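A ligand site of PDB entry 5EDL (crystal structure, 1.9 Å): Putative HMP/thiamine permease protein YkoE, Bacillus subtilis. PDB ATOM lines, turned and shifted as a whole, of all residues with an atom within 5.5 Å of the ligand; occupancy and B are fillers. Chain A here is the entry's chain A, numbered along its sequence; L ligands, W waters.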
ATOM      1  N   TYR A  21      11.111 -10.997 -19.492  1.00  0.00           N
ATOM      2  CA  TYR A  21       9.870 -11.367 -18.831  1.00  0.00           C
ATOM      3  C   TYR A  21       9.910 -12.828 -18.348  1.00  0.00           C
ATOM      4  O   TYR A  21       9.491 -13.141 -17.237  1.00  0.00           O
ATOM      5  CB  TYR A  21       8.672 -11.198 -19.771  1.00  0.00           C
ATOM      6  CG  TYR A  21       8.215  -9.768 -20.020  1.00  0.00           C
ATOM      7  CD1 TYR A  21       8.988  -8.685 -19.626  1.00  0.00           C
ATOM      8  CD2 TYR A  21       7.013  -9.513 -20.658  1.00  0.00           C
ATOM      9  CE1 TYR A  21       8.562  -7.388 -19.839  1.00  0.00           C
ATOM     10  CE2 TYR A  21       6.575  -8.228 -20.876  1.00  0.00           C
ATOM     11  CZ  TYR A  21       7.343  -7.180 -20.465  1.00  0.00           C
ATOM     12  OH  TYR A  21       6.892  -5.916 -20.683  1.00  0.00           O
ATOM     13  N   THR A  25       9.650 -14.237 -14.617  1.00  0.00           N
ATOM     14  CA  THR A  25       8.559 -15.134 -14.278  1.00  0.00           C
ATOM     15  C   THR A  25       9.067 -16.327 -13.480  1.00  0.00           C
ATOM     16  O   THR A  25       8.461 -16.730 -12.479  1.00  0.00           O
ATOM     17  CB  THR A  25       7.817 -15.611 -15.534  1.00  0.00           C
ATOM     18  OG1 THR A  25       6.989 -14.553 -16.003  1.00  0.00           O
ATOM     19  CG2 THR A  25       6.940 -16.829 -15.220  1.00  0.00           C
ATOM     20  N   TYR A  40       6.740 -11.475  -4.962  1.00  0.00           N
ATOM     21  CA  TYR A  40       7.058 -11.004  -6.313  1.00  0.00           C
ATOM     22  C   TYR A  40       6.504  -9.612  -6.625  1.00  0.00           C
ATOM     23  O   TYR A  40       6.736  -9.068  -7.704  1.00  0.00           O
ATOM     24  CB  TYR A  40       6.595 -11.994  -7.390  1.00  0.00           C
ATOM     25  CG  TYR A  40       5.119 -12.334  -7.384  1.00  0.00           C
ATOM     26  CD1 TYR A  40       4.142 -11.346  -7.546  1.00  0.00           C
ATOM     27  CD2 TYR A  40       4.702 -13.646  -7.274  1.00  0.00           C
ATOM     28  CE1 TYR A  40       2.791 -11.664  -7.549  1.00  0.00           C
ATOM     29  CE2 TYR A  40       3.368 -13.980  -7.281  1.00  0.00           C
ATOM     30  CZ  TYR A  40       2.411 -12.995  -7.422  1.00  0.00           C
ATOM     31  OH  TYR A  40       1.084 -13.349  -7.421  1.00  0.00           O
ATOM     32  N   TYR A  44       7.184  -6.586  -9.856  1.00  0.00           N
ATOM     33  CA  TYR A  44       6.064  -6.772 -10.796  1.00  0.00           C
ATOM     34  C   TYR A  44       6.121  -5.827 -11.999  1.00  0.00           C
ATOM     35  O   TYR A  44       5.827  -6.226 -13.116  1.00  0.00           O
ATOM     36  CB  TYR A  44       4.712  -6.602 -10.084  1.00  0.00           C
ATOM     37  CG  TYR A  44       3.656  -7.538 -10.655  1.00  0.00           C
ATOM     38  CD1 TYR A  44       3.109  -7.316 -11.902  1.00  0.00           C
ATOM     39  CD2 TYR A  44       3.250  -8.682  -9.939  1.00  0.00           C
ATOM     40  CE1 TYR A  44       2.164  -8.188 -12.445  1.00  0.00           C
ATOM     41  CE2 TYR A  44       2.304  -9.559 -10.469  1.00  0.00           C
ATOM     42  CZ  TYR A  44       1.771  -9.316 -11.715  1.00  0.00           C
ATOM     43  OH  TYR A  44       0.857 -10.180 -12.253  1.00  0.00           O
ATOM     44  N   TRP A  47       7.272  -6.511 -15.698  1.00  0.00           N
ATOM     45  CA  TRP A  47       6.429  -7.143 -16.722  1.00  0.00           C
ATOM     46  C   TRP A  47       5.599  -6.138 -17.520  1.00  0.00           C
ATOM     47  O   TRP A  47       4.882  -6.543 -18.446  1.00  0.00           O
ATOM     48  CB  TRP A  47       5.489  -8.204 -16.089  1.00  0.00           C
ATOM     49  CG  TRP A  47       6.253  -9.420 -15.620  1.00  0.00           C
ATOM     50  CD1 TRP A  47       7.019 -10.261 -16.378  1.00  0.00           C
ATOM     51  CD2 TRP A  47       6.291  -9.940 -14.287  1.00  0.00           C
ATOM     52  NE1 TRP A  47       7.544 -11.270 -15.587  1.00  0.00           N
ATOM     53  CE2 TRP A  47       7.112 -11.076 -14.298  1.00  0.00           C
ATOM     54  CE3 TRP A  47       5.707  -9.535 -13.070  1.00  0.00           C
ATOM     55  CZ2 TRP A  47       7.366 -11.830 -13.139  1.00  0.00           C
ATOM     56  CZ3 TRP A  47       5.964 -10.267 -11.933  1.00  0.00           C
ATOM     57  CH2 TRP A  47       6.794 -11.407 -11.976  1.00  0.00           C
ATOM     58  N   PHE A  48       5.673  -4.858 -17.159  1.00  0.00           N
ATOM     59  CA  PHE A  48       4.993  -3.804 -17.925  1.00  0.00           C
ATOM     60  C   PHE A  48       5.943  -2.932 -18.770  1.00  0.00           C
ATOM     61  O   PHE A  48       5.489  -2.057 -19.516  1.00  0.00           O
ATOM     62  CB  PHE A  48       4.219  -2.826 -17.020  1.00  0.00           C
ATOM     63  CG  PHE A  48       3.468  -3.465 -15.900  1.00  0.00           C
ATOM     64  CD1 PHE A  48       2.877  -4.707 -16.028  1.00  0.00           C
ATOM     65  CD2 PHE A  48       3.330  -2.787 -14.700  1.00  0.00           C
ATOM     66  CE1 PHE A  48       2.177  -5.271 -14.969  1.00  0.00           C
ATOM     67  CE2 PHE A  48       2.634  -3.324 -13.631  1.00  0.00           C
ATOM     68  CZ  PHE A  48       2.051  -4.581 -13.763  1.00  0.00           C
ATOM     69  N   GLU A  68       3.001  -4.999 -25.637  1.00  0.00           N
ATOM     70  CA  GLU A  68       2.859  -5.897 -24.503  1.00  0.00           C
ATOM     71  C   GLU A  68       2.240  -7.239 -24.924  1.00  0.00           C
ATOM     72  O   GLU A  68       2.623  -8.294 -24.421  1.00  0.00           O
ATOM     73  CB  GLU A  68       2.020  -5.229 -23.397  1.00  0.00           C
ATOM     74  CG  GLU A  68       1.813  -6.037 -22.089  1.00  0.00           C
ATOM     75  CD  GLU A  68       3.046  -6.106 -21.186  1.00  0.00           C
ATOM     76  OE1 GLU A  68       4.128  -5.604 -21.565  1.00  0.00           O
ATOM     77  OE2 GLU A  68       2.950  -6.698 -20.096  1.00  0.00           O
ATOM     78  N   ALA A  71       5.046  -9.172 -26.635  1.00  0.00           N
ATOM     79  CA  ALA A  71       5.967  -9.652 -25.610  1.00  0.00           C
ATOM     80  C   ALA A  71       5.380 -10.860 -24.850  1.00  0.00           C
ATOM     81  O   ALA A  71       6.079 -11.819 -24.591  1.00  0.00           O
ATOM     82  CB  ALA A  71       6.330  -8.507 -24.638  1.00  0.00           C
ATOM     83  N   ALA A  72       4.103 -10.775 -24.491  1.00  0.00           N
ATOM     84  CA  ALA A  72       3.433 -11.862 -23.758  1.00  0.00           C
ATOM     85  C   ALA A  72       3.305 -13.131 -24.615  1.00  0.00           C
ATOM     86  O   ALA A  72       3.485 -14.261 -24.117  1.00  0.00           O
ATOM     87  CB  ALA A  72       2.057 -11.428 -23.274  1.00  0.00           C
ATOM     88  N   GLU A  75       6.724 -14.664 -24.794  1.00  0.00           N
ATOM     89  CA  GLU A  75       7.041 -15.279 -23.505  1.00  0.00           C
ATOM     90  C   GLU A  75       6.324 -16.633 -23.363  1.00  0.00           C
ATOM     91  O   GLU A  75       6.903 -17.604 -22.880  1.00  0.00           O
ATOM     92  CB  GLU A  75       6.667 -14.347 -22.335  1.00  0.00           C
ATOM     93  CG  GLU A  75       7.214 -14.844 -21.008  1.00  0.00           C
ATOM     94  CD  GLU A  75       6.593 -14.143 -19.813  1.00  0.00           C
ATOM     95  OE1 GLU A  75       5.972 -13.075 -20.006  1.00  0.00           O
ATOM     96  OE2 GLU A  75       6.707 -14.681 -18.686  1.00  0.00           O
ATOM     97  N   ASN A  80       6.610 -20.113 -20.927  1.00  0.00           N
ATOM     98  CA  ASN A  80       5.957 -19.698 -19.687  1.00  0.00           C
ATOM     99  C   ASN A  80       5.123 -20.858 -19.140  1.00  0.00           C
ATOM    100  O   ASN A  80       4.250 -21.369 -19.841  1.00  0.00           O
ATOM    101  CB  ASN A  80       5.078 -18.460 -19.905  1.00  0.00           C
ATOM    102  CG  ASN A  80       4.440 -17.955 -18.608  1.00  0.00           C
ATOM    103  OD1 ASN A  80       3.469 -18.531 -18.116  1.00  0.00           O
ATOM    104  ND2 ASN A  80       4.989 -16.892 -18.066  1.00  0.00           N
ATOM    105  N   VAL A  86      -0.826 -16.236 -19.678  1.00  0.00           N
ATOM    106  CA  VAL A  86       0.083 -15.093 -19.618  1.00  0.00           C
ATOM    107  C   VAL A  86      -0.237 -14.108 -20.756  1.00  0.00           C
ATOM    108  O   VAL A  86      -0.007 -12.916 -20.632  1.00  0.00           O
ATOM    109  CB  VAL A  86       1.567 -15.512 -19.677  1.00  0.00           C
ATOM    110  CG1 VAL A  86       1.974 -15.934 -21.103  1.00  0.00           C
ATOM    111  CG2 VAL A  86       2.463 -14.359 -19.192  1.00  0.00           C
ATOM    112  N   ILE A  89      -3.084 -11.946 -19.333  1.00  0.00           N
ATOM    113  CA  ILE A  89      -2.653 -10.886 -18.427  1.00  0.00           C
ATOM    114  C   ILE A  89      -1.838  -9.847 -19.193  1.00  0.00           C
ATOM    115  O   ILE A  89      -1.849  -8.658 -18.862  1.00  0.00           O
ATOM    116  CB  ILE A  89      -1.861 -11.430 -17.197  1.00  0.00           C
ATOM    117  CG1 ILE A  89      -1.981 -10.423 -16.026  1.00  0.00           C
ATOM    118  CG2 ILE A  89      -0.404 -11.735 -17.569  1.00  0.00           C
ATOM    119  CD1 ILE A  89      -1.442 -10.910 -14.681  1.00  0.00           C
ATOM    120  N   GLY A  90      -1.178 -10.291 -20.255  1.00  0.00           N
ATOM    121  CA  GLY A  90      -0.463  -9.365 -21.127  1.00  0.00           C
ATOM    122  C   GLY A  90      -1.406  -8.383 -21.796  1.00  0.00           C
ATOM    123  O   GLY A  90      -1.164  -7.171 -21.792  1.00  0.00           O
ATOM    124  N   GLN A  93      -2.679  -6.003 -19.054  1.00  0.00           N
ATOM    125  CA  GLN A  93      -1.651  -5.036 -18.715  1.00  0.00           C
ATOM    126  C   GLN A  93      -1.467  -3.996 -19.817  1.00  0.00           C
ATOM    127  O   GLN A  93      -1.329  -2.823 -19.524  1.00  0.00           O
ATOM    128  CB  GLN A  93      -0.329  -5.756 -18.393  1.00  0.00           C
ATOM    129  CG  GLN A  93      -0.447  -6.506 -17.053  1.00  0.00           C
ATOM    130  CD  GLN A  93       0.584  -7.613 -16.841  1.00  0.00           C
ATOM    131  OE1 GLN A  93       0.556  -8.281 -15.799  1.00  0.00           O
ATOM    132  NE2 GLN A  93       1.461  -7.830 -17.803  1.00  0.00           N
ATOM    133  N   SER A 125      -3.752  -5.509 -13.899  1.00  0.00           N
ATOM    134  CA  SER A 125      -3.289  -6.837 -13.575  1.00  0.00           C
ATOM    135  C   SER A 125      -3.820  -7.246 -12.203  1.00  0.00           C
ATOM    136  O   SER A 125      -4.072  -8.406 -11.976  1.00  0.00           O
ATOM    137  CB  SER A 125      -1.748  -6.944 -13.615  1.00  0.00           C
ATOM    138  OG  SER A 125      -1.142  -6.066 -12.685  1.00  0.00           O
ATOM    139  N   TYR A 128      -7.251  -8.510 -12.780  1.00  0.00           N
ATOM    140  CA  TYR A 128      -7.103  -9.843 -13.354  1.00  0.00           C
ATOM    141  C   TYR A 128      -6.844 -10.900 -12.268  1.00  0.00           C
ATOM    142  O   TYR A 128      -7.478 -11.963 -12.264  1.00  0.00           O
ATOM    143  CB  TYR A 128      -5.953  -9.855 -14.386  1.00  0.00           C
ATOM    144  CG  TYR A 128      -5.578 -11.239 -14.877  1.00  0.00           C
ATOM    145  CD1 TYR A 128      -4.634 -12.008 -14.206  1.00  0.00           C
ATOM    146  CD2 TYR A 128      -6.155 -11.766 -16.024  1.00  0.00           C
ATOM    147  CE1 TYR A 128      -4.284 -13.285 -14.668  1.00  0.00           C
ATOM    148  CE2 TYR A 128      -5.813 -13.033 -16.489  1.00  0.00           C
ATOM    149  CZ  TYR A 128      -4.876 -13.784 -15.804  1.00  0.00           C
ATOM    150  OH  TYR A 128      -4.523 -15.043 -16.251  1.00  0.00           O
ATOM    151  N   ASP A 129      -5.930 -10.600 -11.364  1.00  0.00           N
ATOM    152  CA  ASP A 129      -5.556 -11.559 -10.320  1.00  0.00           C
ATOM    153  C   ASP A 129      -6.695 -11.877  -9.348  1.00  0.00           C
ATOM    154  O   ASP A 129      -6.796 -12.996  -8.844  1.00  0.00           O
ATOM    155  CB  ASP A 129      -4.348 -11.041  -9.549  1.00  0.00           C
ATOM    156  CG  ASP A 129      -3.066 -11.134 -10.356  1.00  0.00           C
ATOM    157  OD1 ASP A 129      -2.988 -11.961 -11.297  1.00  0.00           O
ATOM    158  OD2 ASP A 129      -2.132 -10.384 -10.032  1.00  0.00           O
ATOM    159  N   SER A 133      -6.226 -15.445 -10.178  1.00  0.00           N
ATOM    160  CA  SER A 133      -5.000 -15.885  -9.524  1.00  0.00           C
ATOM    161  C   SER A 133      -5.134 -16.149  -8.029  1.00  0.00           C
ATOM    162  O   SER A 133      -4.137 -16.227  -7.313  1.00  0.00           O
ATOM    163  CB  SER A 133      -3.895 -14.835  -9.746  1.00  0.00           C
ATOM    164  OG  SER A 133      -3.921 -14.371 -11.077  1.00  0.00           O
ATOM    165  N   TYR A 135      -6.391 -14.236  -5.715  1.00  0.00           N
ATOM    166  CA  TYR A 135      -6.237 -13.066  -4.849  1.00  0.00           C
ATOM    167  C   TYR A 135      -7.502 -12.795  -4.036  1.00  0.00           C
ATOM    168  O   TYR A 135      -7.437 -12.169  -2.981  1.00  0.00           O
ATOM    169  CB  TYR A 135      -5.867 -11.819  -5.664  1.00  0.00           C
ATOM    170  CG  TYR A 135      -4.389 -11.658  -5.864  1.00  0.00           C
ATOM    171  CD1 TYR A 135      -3.578 -12.776  -6.081  1.00  0.00           C
ATOM    172  CD2 TYR A 135      -3.798 -10.403  -5.852  1.00  0.00           C
ATOM    173  CE1 TYR A 135      -2.215 -12.639  -6.272  1.00  0.00           C
ATOM    174  CE2 TYR A 135      -2.432 -10.253  -6.039  1.00  0.00           C
ATOM    175  CZ  TYR A 135      -1.640 -11.364  -6.246  1.00  0.00           C
ATOM    176  OH  TYR A 135      -0.284 -11.209  -6.424  1.00  0.00           O
ATOM    177  N   ARG A 150       2.717  -3.078  -5.779  1.00  0.00           N
ATOM    178  CA  ARG A 150       2.658  -3.230  -7.224  1.00  0.00           C
ATOM    179  C   ARG A 150       2.530  -1.867  -7.920  1.00  0.00           C
ATOM    180  O   ARG A 150       3.072  -1.677  -9.018  1.00  0.00           O
ATOM    181  CB  ARG A 150       1.506  -4.138  -7.669  1.00  0.00           C
ATOM    182  CG  ARG A 150       1.656  -4.587  -9.139  1.00  0.00           C
ATOM    183  CD  ARG A 150       0.503  -5.499  -9.615  1.00  0.00           C
ATOM    184  NE  ARG A 150       0.436  -6.754  -8.842  1.00  0.00           N
ATOM    185  CZ  ARG A 150      -0.376  -7.763  -9.135  1.00  0.00           C
ATOM    186  NH1 ARG A 150      -1.195  -7.687 -10.184  1.00  0.00           N
ATOM    187  NH2 ARG A 150      -0.369  -8.860  -8.385  1.00  0.00           N
HETATM  188  C1  LIG L   1       3.728 -10.592 -19.668  1.00  0.00           C
HETATM  189  N1  LIG L   1       2.367 -10.230 -14.980  1.00  0.00           N
HETATM  190  C2  LIG L   1       3.662 -12.941 -11.199  1.00  0.00           C
HETATM  191  O1  LIG L   1       0.040 -11.935 -10.303  1.00  0.00           O
HETATM  192  C3  LIG L   1      -0.480 -13.240 -10.496  1.00  0.00           C
HETATM  193  C4  LIG L   1       0.691 -14.188 -10.664  1.00  0.00           C
HETATM  194  C5  LIG L   1       1.675 -13.686 -14.470  1.00  0.00           C
HETATM  195  S1  LIG L   1       0.627 -14.143 -13.410  1.00  0.00           S
HETATM  196  C6  LIG L   1       1.294 -13.908 -12.028  1.00  0.00           C
HETATM  197  C7  LIG L   1       2.610 -13.342 -12.245  1.00  0.00           C
HETATM  198  N2  LIG L   1       2.845 -13.214 -13.786  1.00  0.00           N
HETATM  199  C8  LIG L   1       4.109 -12.698 -14.317  1.00  0.00           C
HETATM  200  C9  LIG L   1       3.114 -10.910 -16.019  1.00  0.00           C
HETATM  201  N3  LIG L   1       3.083 -10.479 -17.279  1.00  0.00           N
HETATM  202  C10 LIG L   1       3.803 -11.139 -18.237  1.00  0.00           C
HETATM  203  N4  LIG L   1       4.565 -12.224 -17.893  1.00  0.00           N
HETATM  204  C11 LIG L   1       4.602 -12.678 -16.611  1.00  0.00           C
HETATM  205  C12 LIG L   1       3.874 -12.003 -15.671  1.00  0.00           C
HETATM  206  O   HOH W   1       0.417 -15.876 -16.317  1.00  0.00           O
HETATM  207  O   HOH W   2       3.356 -15.848 -16.088  1.00  0.00           O
HETATM  208  O   HOH W   3       4.038 -16.217 -13.464  1.00  0.00           O
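Tyr 21 touches the ligand (CD2 to C1, 3.6 Å).
Thr 25 touches the ligand.
CE2 of Trp 47 touches C8 of the ligand (3.4 Å).
Glu 68 touches the ligand.
Val 86 touches the ligand (CG2 to N4, 3.3 Å).
CG2 of Ile 89 touches N3 of the ligand, 3.7 Å away.
Ser 133 touches the ligand.
OH of Tyr 135 touches O1 of the ligand, at 3.96 Å.
Arg 150 touches the ligand (NH2 to O1, 3.6 Å).
Hydrophobic or aromatic side chains within 4 Å of the ligand: Tyr 21, Tyr 40, Tyr 44, Trp 47, Val 86 and Ile 89.
Within 4 Å of the ligand: Tyr 21, Thr 25, Tyr 40, Tyr 44, Trp 47, Glu 68, Glu 75, Val 86, Ile 89, Gln 93, Asp 129, Ser 133, Tyr 135 and Arg 150.
The side-chain carboxylate of Glu 75 lies within hydrogen-bond range of the side-chain hydroxyl of Thr 25 (2.7 Å).
The side-chain carboxylate (OD2) of Asp 129 is in salt-bridge range of the guanidinium group (NH2) of Arg 150 (2.9 Å).
The side-chain hydroxyl (OG1) of Thr 25 sits at hydrogen-bond distance from the indole nitrogen (NE1) of Trp 47 (3.4 Å).
The side-chain hydroxyl (OH) of Tyr 40 lies within hydrogen-bond range of the side-chain hydroxyl (OH) of Tyr 135 (2.7 Å).
The backbone carbonyl oxygen of Trp 47 lies within hydrogen-bond range of the side-chain hydroxyl of Tyr 21 (3.1 Å).
OH of Tyr 21 sits at hydrogen-bond distance from OE1 of Glu 68, 2.9 Å away.
NH2 of Arg 150 is in hydrogen-bond range of OH of Tyr 135, 3.1 Å away.
The guanidinium group of Arg 150 sits at hydrogen-bond distance from the side-chain hydroxyl of Ser 125 (3.0 Å).
OE1 of Glu 75 lies within hydrogen-bond range of N4 of the ligand (2.7 Å).
OD2 of Asp 129 lies within hydrogen-bond range of O1 of the ligand.
The side-chain hydroxyl of Tyr 44 lies within hydrogen-bond range of an oxygen (O1) of the ligand.
A nitrogen (N1) of the ligand sits at hydrogen-bond distance from the side-chain amide oxygen (OE1) of Gln 93 (2.8 Å).
The side-chain hydroxyl (OH) of Tyr 40 sits close to an oxygen (O1) of the ligand (3.4 Å).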
